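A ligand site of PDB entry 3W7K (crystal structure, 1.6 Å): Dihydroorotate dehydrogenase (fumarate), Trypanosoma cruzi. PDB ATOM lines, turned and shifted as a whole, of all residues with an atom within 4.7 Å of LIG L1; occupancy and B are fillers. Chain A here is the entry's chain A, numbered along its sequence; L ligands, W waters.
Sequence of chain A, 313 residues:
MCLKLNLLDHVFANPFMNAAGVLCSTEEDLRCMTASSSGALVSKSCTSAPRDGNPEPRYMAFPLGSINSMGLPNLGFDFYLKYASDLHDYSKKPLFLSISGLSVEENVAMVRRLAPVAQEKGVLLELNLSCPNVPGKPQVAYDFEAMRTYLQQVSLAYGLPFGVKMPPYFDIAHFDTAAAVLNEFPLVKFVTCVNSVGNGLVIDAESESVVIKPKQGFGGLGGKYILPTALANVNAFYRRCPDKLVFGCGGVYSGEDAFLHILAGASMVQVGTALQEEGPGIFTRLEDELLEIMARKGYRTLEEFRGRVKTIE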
ATOM      1  N   ALA A  19       2.994 -13.363  14.290  1.00  0.00           N
ATOM      2  CA  ALA A  19       4.168 -12.597  14.707  1.00  0.00           C
ATOM      3  C   ALA A  19       5.316 -12.763  13.696  1.00  0.00           C
ATOM      4  O   ALA A  19       5.448 -13.824  13.118  1.00  0.00           O
ATOM      5  CB  ALA A  19       4.600 -13.146  16.070  1.00  0.00           C
ATOM      6  N   ALA A  20       6.109 -11.747  13.481  1.00  0.00           N
ATOM      7  CA  ALA A  20       7.193 -11.903  12.558  1.00  0.00           C
ATOM      8  C   ALA A  20       8.075 -13.114  12.927  1.00  0.00           C
ATOM      9  O   ALA A  20       8.349 -13.336  14.086  1.00  0.00           O
ATOM     10  CB  ALA A  20       8.021 -10.652  12.469  1.00  0.00           C
ATOM     11  N   GLY A  21       8.467 -13.873  11.917  1.00  0.00           N
ATOM     12  CA  GLY A  21       9.250 -15.022  12.065  1.00  0.00           C
ATOM     13  C   GLY A  21       8.493 -16.284  11.994  1.00  0.00           C
ATOM     14  O   GLY A  21       9.092 -17.354  11.760  1.00  0.00           O
ATOM     15  N   VAL A  22       7.207 -16.262  12.379  1.00  0.00           N
ATOM     16  CA  VAL A  22       6.425 -17.521  12.383  1.00  0.00           C
ATOM     17  C   VAL A  22       5.569 -17.549  11.119  1.00  0.00           C
ATOM     18  O   VAL A  22       4.774 -16.654  10.857  1.00  0.00           O
ATOM     19  CB  VAL A  22       5.581 -17.574  13.678  1.00  0.00           C
ATOM     20  CG1 VAL A  22       4.668 -18.758  13.693  1.00  0.00           C
ATOM     21  CG2 VAL A  22       6.513 -17.549  14.896  1.00  0.00           C
ATOM     22  N   LYS A  44       8.815 -12.539   7.349  1.00  0.00           N
ATOM     23  CA  LYS A  44       9.993 -12.803   8.089  1.00  0.00           C
ATOM     24  C   LYS A  44      10.907 -11.622   8.038  1.00  0.00           C
ATOM     25  O   LYS A  44      11.183 -11.123   6.972  1.00  0.00           O
ATOM     26  CB  LYS A  44      10.687 -14.034   7.590  1.00  0.00           C
ATOM     27  CG  LYS A  44      12.044 -14.267   8.192  1.00  0.00           C
ATOM     28  CD  LYS A  44      12.092 -14.658   9.673  1.00  0.00           C
ATOM     29  CE  LYS A  44      13.490 -14.563  10.337  1.00  0.00           C
ATOM     30  NZ  LYS A  44      13.463 -14.931  11.813  1.00  0.00           N
ATOM     31  N   SER A  45      11.410 -11.235   9.188  1.00  0.00           N
ATOM     32  CA  SER A  45      12.408 -10.116   9.247  1.00  0.00           C
ATOM     33  C   SER A  45      13.518 -10.483   8.282  1.00  0.00           C
ATOM     34  O   SER A  45      14.050 -11.546   8.328  1.00  0.00           O
ATOM     35  CB  SER A  45      12.994  -9.873  10.605  1.00  0.00           C
ATOM     36  OG  SER A  45      12.019  -9.392  11.489  1.00  0.00           O
ATOM     37  N   TYR A  59      14.995 -24.008  17.457  1.00  0.00           N
ATOM     38  CA  TYR A  59      13.695 -23.737  18.075  1.00  0.00           C
ATOM     39  C   TYR A  59      13.201 -24.975  18.769  1.00  0.00           C
ATOM     40  O   TYR A  59      13.209 -26.089  18.177  1.00  0.00           O
ATOM     41  CB  TYR A  59      12.682 -23.380  16.936  1.00  0.00           C
ATOM     42  CG  TYR A  59      11.237 -23.280  17.393  1.00  0.00           C
ATOM     43  CD1 TYR A  59      10.375 -24.359  17.310  1.00  0.00           C
ATOM     44  CD2 TYR A  59      10.715 -22.127  17.918  1.00  0.00           C
ATOM     45  CE1 TYR A  59       9.099 -24.276  17.859  1.00  0.00           C
ATOM     46  CE2 TYR A  59       9.415 -22.021  18.363  1.00  0.00           C
ATOM     47  CZ  TYR A  59       8.577 -23.091  18.326  1.00  0.00           C
ATOM     48  OH  TYR A  59       7.275 -23.021  18.778  1.00  0.00           O
ATOM     49  N   SER A  66       8.134 -21.365  24.176  1.00  0.00           N
ATOM     50  CA  SER A  66       9.180 -21.713  23.241  1.00  0.00           C
ATOM     51  C   SER A  66      10.489 -20.940  23.561  1.00  0.00           C
ATOM     52  O   SER A  66      10.537 -19.873  24.173  1.00  0.00           O
ATOM     53  CB  SER A  66       8.772 -21.433  21.779  1.00  0.00           C
ATOM     54  OG  SER A  66       8.696 -19.998  21.577  1.00  0.00           O
ATOM     55  N   ASN A  68      14.061 -19.874  21.116  1.00  0.00           N
ATOM     56  CA  ASN A  68      14.633 -19.869  19.784  1.00  0.00           C
ATOM     57  C   ASN A  68      15.904 -19.105  19.703  1.00  0.00           C
ATOM     58  O   ASN A  68      16.063 -18.053  20.321  1.00  0.00           O
ATOM     59  CB  ASN A  68      13.651 -19.399  18.700  1.00  0.00           C
ATOM     60  CG  ASN A  68      13.653 -17.911  18.524  1.00  0.00           C
ATOM     61  OD1 ASN A  68      14.485 -17.355  17.764  1.00  0.00           O
ATOM     62  ND2 ASN A  68      12.735 -17.173  19.161  1.00  0.00           N
ATOM     63  N   MET A  70      16.994 -18.581  16.169  1.00  0.00           N
ATOM     64  CA  MET A  70      16.947 -18.846  14.752  1.00  0.00           C
ATOM     65  C   MET A  70      18.134 -18.252  13.988  1.00  0.00           C
ATOM     66  O   MET A  70      18.680 -18.858  13.053  1.00  0.00           O
ATOM     67  CB  MET A  70      15.673 -18.314  14.150  1.00  0.00           C
ATOM     68  CG  MET A  70      14.339 -18.820  14.663  1.00  0.00           C
ATOM     69  SD  MET A  70      14.188 -20.606  14.699  1.00  0.00           S
ATOM     70  CE  MET A  70      14.035 -20.910  13.040  1.00  0.00           C
ATOM     71  N   LEU A  72      17.990 -15.214  12.215  1.00  0.00           N
ATOM     72  CA  LEU A  72      17.476 -14.479  11.057  1.00  0.00           C
ATOM     73  C   LEU A  72      17.679 -15.294   9.730  1.00  0.00           C
ATOM     74  O   LEU A  72      18.085 -14.758   8.691  1.00  0.00           O
ATOM     75  CB  LEU A  72      18.152 -13.103  10.926  1.00  0.00           C
ATOM     76  CG  LEU A  72      17.486 -11.810  10.580  1.00  0.00           C
ATOM     77  CD1 LEU A  72      16.105 -11.606  11.179  1.00  0.00           C
ATOM     78  CD2 LEU A  72      18.485 -10.679  11.030  1.00  0.00           C
ATOM     79  N   SER A  98       8.610  -6.975   7.475  1.00  0.00           N
ATOM     80  CA  SER A  98       9.549  -6.730   8.580  1.00  0.00           C
ATOM     81  C   SER A  98      10.979  -6.702   8.091  1.00  0.00           C
ATOM     82  O   SER A  98      11.380  -7.564   7.314  1.00  0.00           O
ATOM     83  CB  SER A  98       9.381  -7.770   9.675  1.00  0.00           C
ATOM     84  OG  SER A  98      10.367  -7.497  10.674  1.00  0.00           O
ATOM     85  N   GLU A 126       7.413  -2.786   9.214  1.00  0.00           N
ATOM     86  CA  GLU A 126       7.709  -3.014  10.635  1.00  0.00           C
ATOM     87  C   GLU A 126       9.223  -3.157  10.732  1.00  0.00           C
ATOM     88  O   GLU A 126       9.825  -4.137  10.227  1.00  0.00           O
ATOM     89  CB  GLU A 126       6.942  -4.282  11.193  1.00  0.00           C
ATOM     90  CG  GLU A 126       7.198  -4.506  12.705  1.00  0.00           C
ATOM     91  CD  GLU A 126       6.378  -5.707  13.335  1.00  0.00           C
ATOM     92  OE1 GLU A 126       6.926  -6.832  13.285  1.00  0.00           O
ATOM     93  OE2 GLU A 126       5.239  -5.567  13.902  1.00  0.00           O
ATOM     94  N   ASN A 128      12.452  -4.000  12.833  1.00  0.00           N
ATOM     95  CA  ASN A 128      12.861  -4.724  13.977  1.00  0.00           C
ATOM     96  C   ASN A 128      14.016  -4.120  14.722  1.00  0.00           C
ATOM     97  O   ASN A 128      15.109  -4.131  14.234  1.00  0.00           O
ATOM     98  CB  ASN A 128      13.177  -6.151  13.562  1.00  0.00           C
ATOM     99  CG  ASN A 128      13.346  -7.060  14.756  1.00  0.00           C
ATOM    100  OD1 ASN A 128      13.218  -6.688  15.883  1.00  0.00           O
ATOM    101  ND2 ASN A 128      13.603  -8.309  14.423  1.00  0.00           N
ATOM    102  N   LYS A 165       9.197  -2.820  15.968  1.00  0.00           N
ATOM    103  CA  LYS A 165       9.046  -4.001  16.859  1.00  0.00           C
ATOM    104  C   LYS A 165      10.024  -3.854  17.980  1.00  0.00           C
ATOM    105  O   LYS A 165      11.243  -3.734  17.769  1.00  0.00           O
ATOM    106  CB  LYS A 165       9.344  -5.263  16.092  1.00  0.00           C
ATOM    107  CG  LYS A 165       9.271  -6.587  16.893  1.00  0.00           C
ATOM    108  CD  LYS A 165       7.880  -7.067  17.179  1.00  0.00           C
ATOM    109  CE  LYS A 165       7.859  -8.480  17.687  1.00  0.00           C
ATOM    110  NZ  LYS A 165       8.116  -9.468  16.672  1.00  0.00           N
ATOM    111  N   VAL A 194       5.518  -7.379  22.283  1.00  0.00           N
ATOM    112  CA  VAL A 194       6.948  -7.378  22.429  1.00  0.00           C
ATOM    113  C   VAL A 194       7.533  -8.489  21.554  1.00  0.00           C
ATOM    114  O   VAL A 194       6.902  -9.489  21.220  1.00  0.00           O
ATOM    115  CB  VAL A 194       7.452  -7.606  23.914  1.00  0.00           C
ATOM    116  CG1 VAL A 194       7.036  -6.447  24.753  1.00  0.00           C
ATOM    117  CG2 VAL A 194       6.849  -8.911  24.458  1.00  0.00           C
ATOM    118  N   ASN A 195       8.810  -8.309  21.251  1.00  0.00           N
ATOM    119  CA  ASN A 195       9.703  -9.433  20.763  1.00  0.00           C
ATOM    120  C   ASN A 195       9.918 -10.453  21.907  1.00  0.00           C
ATOM    121  O   ASN A 195       9.434 -10.247  23.072  1.00  0.00           O
ATOM    122  CB  ASN A 195      11.016  -8.819  20.225  1.00  0.00           C
ATOM    123  CG  ASN A 195      11.572  -9.615  19.072  1.00  0.00           C
ATOM    124  OD1 ASN A 195      11.699 -10.801  19.156  1.00  0.00           O
ATOM    125  ND2 ASN A 195      11.847  -8.959  17.966  1.00  0.00           N
ATOM    126  N   SER A 196      10.668 -11.526  21.617  1.00  0.00           N
ATOM    127  CA  SER A 196      10.960 -12.534  22.630  1.00  0.00           C
ATOM    128  C   SER A 196      11.689 -11.968  23.802  1.00  0.00           C
ATOM    129  O   SER A 196      12.379 -10.942  23.729  1.00  0.00           O
ATOM    130  CB  SER A 196      11.654 -13.720  21.925  1.00  0.00           C
ATOM    131  OG  SER A 196      12.760 -13.217  21.285  1.00  0.00           O
ATOM    132  N   GLY A 222       9.269 -17.195  24.157  1.00  0.00           N
ATOM    133  CA  GLY A 222       7.944 -16.817  23.810  1.00  0.00           C
ATOM    134  C   GLY A 222       6.921 -17.690  24.521  1.00  0.00           C
ATOM    135  O   GLY A 222       7.265 -18.703  25.141  1.00  0.00           O
ATOM    136  N   GLY A 223       5.674 -17.348  24.355  1.00  0.00           N
ATOM    137  CA  GLY A 223       4.590 -18.117  24.789  1.00  0.00           C
ATOM    138  C   GLY A 223       4.048 -17.773  26.164  1.00  0.00           C
ATOM    139  O   GLY A 223       4.109 -16.617  26.589  1.00  0.00           O
ATOM    140  N   ILE A 226       5.641 -15.412  28.868  1.00  0.00           N
ATOM    141  CA  ILE A 226       5.866 -13.974  28.640  1.00  0.00           C
ATOM    142  C   ILE A 226       4.591 -13.104  28.612  1.00  0.00           C
ATOM    143  O   ILE A 226       4.714 -11.890  28.445  1.00  0.00           O
ATOM    144  CB  ILE A 226       6.708 -13.745  27.368  1.00  0.00           C
ATOM    145  CG1 ILE A 226       5.976 -13.805  26.052  1.00  0.00           C
ATOM    146  CG2 ILE A 226       7.972 -14.617  27.405  1.00  0.00           C
ATOM    147  CD1 ILE A 226       6.708 -13.097  24.914  1.00  0.00           C
ATOM    148  N   CYS A 249       1.957  -8.376  21.139  1.00  0.00           N
ATOM    149  CA  CYS A 249       2.515  -9.638  20.737  1.00  0.00           C
ATOM    150  C   CYS A 249       3.096 -10.244  22.037  1.00  0.00           C
ATOM    151  O   CYS A 249       3.808  -9.587  22.799  1.00  0.00           O
ATOM    152  CB  CYS A 249       3.626  -9.456  19.722  1.00  0.00           C
ATOM    153  SG  CYS A 249       4.283 -11.016  19.061  1.00  0.00           S
ATOM    154  N   GLY A 250       2.773 -11.458  22.323  1.00  0.00           N
ATOM    155  CA  GLY A 250       3.389 -12.248  23.403  1.00  0.00           C
ATOM    156  C   GLY A 250       2.357 -13.025  24.194  1.00  0.00           C
ATOM    157  O   GLY A 250       1.436 -12.448  24.794  1.00  0.00           O
ATOM    158  N   GLY A 251       2.516 -14.342  24.180  1.00  0.00           N
ATOM    159  CA  GLY A 251       1.647 -15.148  25.028  1.00  0.00           C
ATOM    160  C   GLY A 251       0.241 -15.328  24.628  1.00  0.00           C
ATOM    161  O   GLY A 251      -0.542 -15.773  25.454  1.00  0.00           O
ATOM    162  N   VAL A 252      -0.107 -15.078  23.371  1.00  0.00           N
ATOM    163  CA  VAL A 252      -1.498 -15.248  22.947  1.00  0.00           C
ATOM    164  C   VAL A 252      -1.725 -16.699  22.512  1.00  0.00           C
ATOM    165  O   VAL A 252      -1.188 -17.136  21.473  1.00  0.00           O
ATOM    166  CB  VAL A 252      -1.926 -14.256  21.803  1.00  0.00           C
ATOM    167  CG1 VAL A 252      -3.322 -14.544  21.343  1.00  0.00           C
ATOM    168  CG2 VAL A 252      -1.733 -12.822  22.307  1.00  0.00           C
ATOM    169  N   GLN A 270      -0.704 -10.058  17.643  1.00  0.00           N
ATOM    170  CA  GLN A 270       0.146 -10.977  16.857  1.00  0.00           C
ATOM    171  C   GLN A 270       0.325 -12.277  17.681  1.00  0.00           C
ATOM    172  O   GLN A 270       0.287 -12.263  18.914  1.00  0.00           O
ATOM    173  CB  GLN A 270       1.519 -10.360  16.596  1.00  0.00           C
ATOM    174  CG  GLN A 270       1.475  -8.961  16.047  1.00  0.00           C
ATOM    175  CD  GLN A 270       2.797  -8.467  15.584  1.00  0.00           C
ATOM    176  OE1 GLN A 270       3.809  -8.887  16.116  1.00  0.00           O
ATOM    177  NE2 GLN A 270       2.786  -7.520  14.662  1.00  0.00           N
ATOM    178  N   VAL A 271       0.456 -13.379  16.945  1.00  0.00           N
ATOM    179  CA  VAL A 271       0.500 -14.757  17.430  1.00  0.00           C
ATOM    180  C   VAL A 271       1.735 -15.411  16.910  1.00  0.00           C
ATOM    181  O   VAL A 271       1.870 -15.636  15.726  1.00  0.00           O
ATOM    182  CB  VAL A 271      -0.785 -15.491  17.036  1.00  0.00           C
ATOM    183  CG1 VAL A 271      -0.755 -16.773  17.831  1.00  0.00           C
ATOM    184  CG2 VAL A 271      -2.024 -14.628  17.367  1.00  0.00           C
ATOM    185  N   GLY A 272       2.649 -15.758  17.833  1.00  0.00           N
ATOM    186  CA  GLY A 272       3.936 -16.388  17.470  1.00  0.00           C
ATOM    187  C   GLY A 272       3.916 -17.879  17.869  1.00  0.00           C
ATOM    188  O   GLY A 272       3.473 -18.726  17.113  1.00  0.00           O
ATOM    189  N   THR A 273       4.438 -18.167  19.052  1.00  0.00           N
ATOM    190  CA  THR A 273       4.537 -19.579  19.537  1.00  0.00           C
ATOM    191  C   THR A 273       3.277 -20.339  19.353  1.00  0.00           C
ATOM    192  O   THR A 273       3.354 -21.452  18.838  1.00  0.00           O
ATOM    193  CB  THR A 273       4.937 -19.558  21.025  1.00  0.00           C
ATOM    194  OG1 THR A 273       6.177 -18.919  21.153  1.00  0.00           O
ATOM    195  CG2 THR A 273       5.050 -20.947  21.594  1.00  0.00           C
HETATM  196  N1  LIG L   1      10.465 -11.329  15.797  1.00  0.00           N
HETATM  197  C1  LIG L   1      10.814 -10.500  14.811  1.00  0.00           C
HETATM  198  O1  LIG L   1      10.451  -9.314  14.930  1.00  0.00           O
HETATM  199  N2  LIG L   1      11.399 -10.921  13.687  1.00  0.00           N
HETATM  200  C2  LIG L   1      11.664 -12.257  13.473  1.00  0.00           C
HETATM  201  O2  LIG L   1      12.165 -12.642  12.382  1.00  0.00           O
HETATM  202  C3  LIG L   1      11.375 -13.186  14.500  1.00  0.00           C
HETATM  203  N3  LIG L   1      11.605 -14.502  14.319  1.00  0.00           N
HETATM  204  C4  LIG L   1      11.078 -15.412  15.213  1.00  0.00           C
HETATM  205  C5  LIG L   1      11.152 -16.774  14.945  1.00  0.00           C
HETATM  206  C6  LIG L   1      10.686 -17.698  15.831  1.00  0.00           C
HETATM  207  C7  LIG L   1      10.757 -19.154  15.527  1.00  0.00           C
HETATM  208  C8  LIG L   1       9.975 -17.218  16.980  1.00  0.00           C
HETATM  209  C9  LIG L   1       9.415 -18.174  17.935  1.00  0.00           C
HETATM  210  C10 LIG L   1       9.865 -15.853  17.238  1.00  0.00           C
HETATM  211  C11 LIG L   1      10.411 -14.928  16.384  1.00  0.00           C
HETATM  212  N4  LIG L   1      10.289 -13.541  16.623  1.00  0.00           N
HETATM  213  C12 LIG L   1      10.660 -12.653  15.628  1.00  0.00           C
HETATM  214  C13 LIG L   1       9.588 -13.054  17.799  1.00  0.00           C
HETATM  215  C14 LIG L   1       8.064 -13.214  17.642  1.00  0.00           C
HETATM  216  O3  LIG L   1       7.710 -12.303  16.587  1.00  0.00           O
HETATM  217  C15 LIG L   1       7.378 -12.745  18.901  1.00  0.00           C
HETATM  218  O4  LIG L   1       7.706 -11.346  19.166  1.00  0.00           O
HETATM  219  C16 LIG L   1       7.729 -13.635  20.136  1.00  0.00           C
HETATM  220  O5  LIG L   1       7.810 -15.007  19.710  1.00  0.00           O
HETATM  221  C17 LIG L   1       6.641 -13.434  21.210  1.00  0.00           C
HETATM  222  O6  LIG L   1       5.345 -13.819  20.786  1.00  0.00           O
HETATM  223  P1  LIG L   1       4.736 -15.254  21.285  1.00  0.00           P
HETATM  224  O7  LIG L   1       3.405 -15.291  20.599  1.00  0.00           O
HETATM  225  O8  LIG L   1       4.731 -15.284  22.755  1.00  0.00           O
HETATM  226  O9  LIG L   1       5.706 -16.333  20.724  1.00  0.00           O
HETATM  227  O1  LG2 L   2      15.683 -14.529  13.841  1.00  0.00           O
HETATM  228  C1  LG2 L   2      15.791 -14.586  15.082  1.00  0.00           C
HETATM  229  O2  LG2 L   2      16.672 -15.305  15.599  1.00  0.00           O
HETATM  230  C2  LG2 L   2      14.938 -13.847  15.895  1.00  0.00           C
HETATM  231  N1  LG2 L   2      14.276 -14.464  16.968  1.00  0.00           N
HETATM  232  C3  LG2 L   2      13.417 -13.720  17.775  1.00  0.00           C
HETATM  233  O3  LG2 L   2      12.833 -14.259  18.717  1.00  0.00           O
HETATM  234  N2  LG2 L   2      13.221 -12.359  17.524  1.00  0.00           N
HETATM  235  C4  LG2 L   2      13.882 -11.742  16.451  1.00  0.00           C
HETATM  236  O4  LG2 L   2      13.709 -10.544  16.231  1.00  0.00           O
HETATM  237  C5  LG2 L   2      14.735 -12.494  15.645  1.00  0.00           C
HETATM  238  C6  LG2 L   2      15.403 -11.882  14.579  1.00  0.00           C
HETATM  239  C7  LG2 L   2      16.510 -10.978  15.134  1.00  0.00           C
HETATM  240  C8  LG2 L   2      17.536 -11.756  15.638  1.00  0.00           C
HETATM  241  C9  LG2 L   2      18.637 -12.085  14.839  1.00  0.00           C
HETATM  242  C10 LG2 L   2      19.665 -12.864  15.358  1.00  0.00           C
HETATM  243  C11 LG2 L   2      20.755 -13.183  14.560  1.00  0.00           C
HETATM  244  C12 LG2 L   2      21.787 -13.967  15.071  1.00  0.00           C
HETATM  245  C13 LG2 L   2      21.722 -14.425  16.372  1.00  0.00           C
HETATM  246  O5  LG2 L   2      22.731 -15.190  16.872  1.00  0.00           O
HETATM  247  C14 LG2 L   2      23.686 -15.455  15.851  1.00  0.00           C
HETATM  248  C15 LG2 L   2      20.627 -14.101  17.178  1.00  0.00           C
HETATM  249  C16 LG2 L   2      19.606 -13.327  16.666  1.00  0.00           C
HETATM  250  C17 LG2 L   2      18.511 -13.003  17.471  1.00  0.00           C
HETATM  251  C18 LG2 L   2      17.488 -12.229  16.945  1.00  0.00           C
HETATM  252  O6  LG2 L   2      16.397 -11.876  17.671  1.00  0.00           O
HETATM  253  C19 LG2 L   2      16.671 -12.048  19.060  1.00  0.00           C
HETATM  254  O   HOH W   1       9.753 -15.838  20.941  1.00  0.00           O
HETATM  255  O   HOH W   2       1.368 -13.630  21.109  1.00  0.00           O
HETATM  256  O   HOH W   3      12.179 -17.539  11.733  1.00  0.00           O
HETATM  257  O   HOH W   4       9.576  -7.290  13.135  1.00  0.00           O
HETATM  258  O   HOH W   5       1.744 -17.340  21.138  1.00  0.00           O
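Ala 19 touches LIG L1.
Gly 21 touches LIG L1 (CA to N3, 3.3 Å).
CD2 of Tyr 59 touches C7 of LIG L1, 3.8 Å away.
ND2 of Asn 68 touches C8 of LIG L1, 3.5 Å away.
Met 70 touches LIG L1 (CG to C7, 3.7 Å).
N of Ser 196 touches O4 of LIG L1, at 3.8 Å.
C of Gly 222 touches O8 of LIG L1, 3.7 Å away.
CD1 of Ile 226 touches O8 of LIG L1, 3.7 Å away.
Gly 250 touches LIG L1 (CA to O8, 3.4 Å).
Hydrophobic or aromatic side chains within 4 Å of LIG L1: Ala 19, Ala 20, Tyr 59, Met 70 and Ile 226.
21 residues have an atom within 4 Å of LIG L1: Ala 19, Ala 20, Gly 21, Lys 44, Ser 45, Tyr 59, Asn 68, Met 70, Asn 128, Lys 165, Val 194, Asn 195, Ser 196, Gly 222, Gly 223, Ile 226, Cys 249, Gly 250, Gly 251, Gly 272 and Thr 273.
The nearest printed residue that does not touch LIG L1 is Val 271 (4.1 Å).
N1 of LIG L1 sits close to N2 of LG2 L2 (3.4 Å).
Water W5 bridges O7 of LIG L1 (2.7 Å) and O of Val 252 (3.0 Å).
Water W4 lies within hydrogen-bond range of OG of Ser 98 (2.6 Å), OE1 of Glu 126 (2.7 Å) and O1 of LIG L1 (2.8 Å).
Water W3 bridges NZ of Lys 44 (2.9 Å) and O of Gly 21 (3.1 Å).
The side-chain amide oxygen of Asn 195 sits at hydrogen-bond distance from a nitrogen (N2) of LG2 L2.
The backbone NH (N) of Met 70 lies within hydrogen-bond range of an oxygen (O2) of LG2 L2 (3.3 Å).
N of Gly 272 is in hydrogen-bond range of O7 of LIG L1, at 2.9 Å.
O of Ala 20 is in hydrogen-bond range of O3 of LIG L1 (2.8 Å).
An oxygen (O9) of LIG L1 is in hydrogen-bond range of the side-chain hydroxyl (OG1) of Thr 273 (2.7 Å).
A nitrogen (N2) of LIG L1 is in hydrogen-bond range of the side-chain hydroxyl of Ser 45 (2.7 Å).
The side-chain amino group (NZ) of Lys 165 is in hydrogen-bond range of an oxygen (O3) of LIG L1, at 2.9 Å.
N of Thr 273 sits at hydrogen-bond distance from O9 of LIG L1 (2.8 Å).
The backbone NH (N) of Gly 223 sits at hydrogen-bond distance from an oxygen (O8) of LIG L1, at 2.8 Å.
An oxygen (O3) of LG2 L2 sits at hydrogen-bond distance from the side-chain hydroxyl of Ser 196 (2.8 Å).
An oxygen (O2) of LIG L1 lies within hydrogen-bond range of the side-chain amino group (NZ) of Lys 44.
The side-chain amide nitrogen (ND2) of Asn 128 is in hydrogen-bond range of an oxygen (O1) of LIG L1 (3.3 Å).
O1 of LG2 L2 is in salt-bridge range of NZ of Lys 44.
An oxygen (O4) of LIG L1 lies within hydrogen-bond range of the side-chain sulfur (SG) of Cys 249.
The backbone carbonyl oxygen of Val 194 is in hydrogen-bond range of an oxygen (O4) of LIG L1 (2.9 Å).
ND2 of Asn 68 is in hydrogen-bond range of O3 of LG2 L2.
ND2 of Asn 128 lies within hydrogen-bond range of O4 of LG2 L2 (2.9 Å).
An oxygen (O1) of LG2 L2 is in hydrogen-bond range of the backbone NH of Leu 72 (2.9 Å).
The backbone NH of Gly 251 sits at hydrogen-bond distance from an oxygen (O8) of LIG L1 (2.8 Å).
O1 of LIG L1 lies within hydrogen-bond range of ND2 of Asn 195, at 3.4 Å.
ND2 of Asn 195 lies within hydrogen-bond range of OD1 of Asn 128.
The side-chain sulfur (SG) of Cys 249 lies close to the side-chain amide oxygen (OE1) of Gln 270 (3.7 Å).
N of Ala 19 is in hydrogen-bond range of O of Val 271.
OG of Ser 66 lies within hydrogen-bond range of OG1 of Thr 273 (2.8 Å).
The backbone NH (N) of Ser 66 sits at hydrogen-bond distance from the backbone carbonyl oxygen (O) of Gly 222.
OG of Ser 98 is in hydrogen-bond range of OG of Ser 45 (2.6 Å).
OD1 of Asn 68 sits at hydrogen-bond distance from N of Met 70 (3.2 Å).
The side-chain hydroxyl (OG) of Ser 196 lies within hydrogen-bond range of the side-chain amide oxygen (OD1) of Asn 195, 3.4 Å away.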
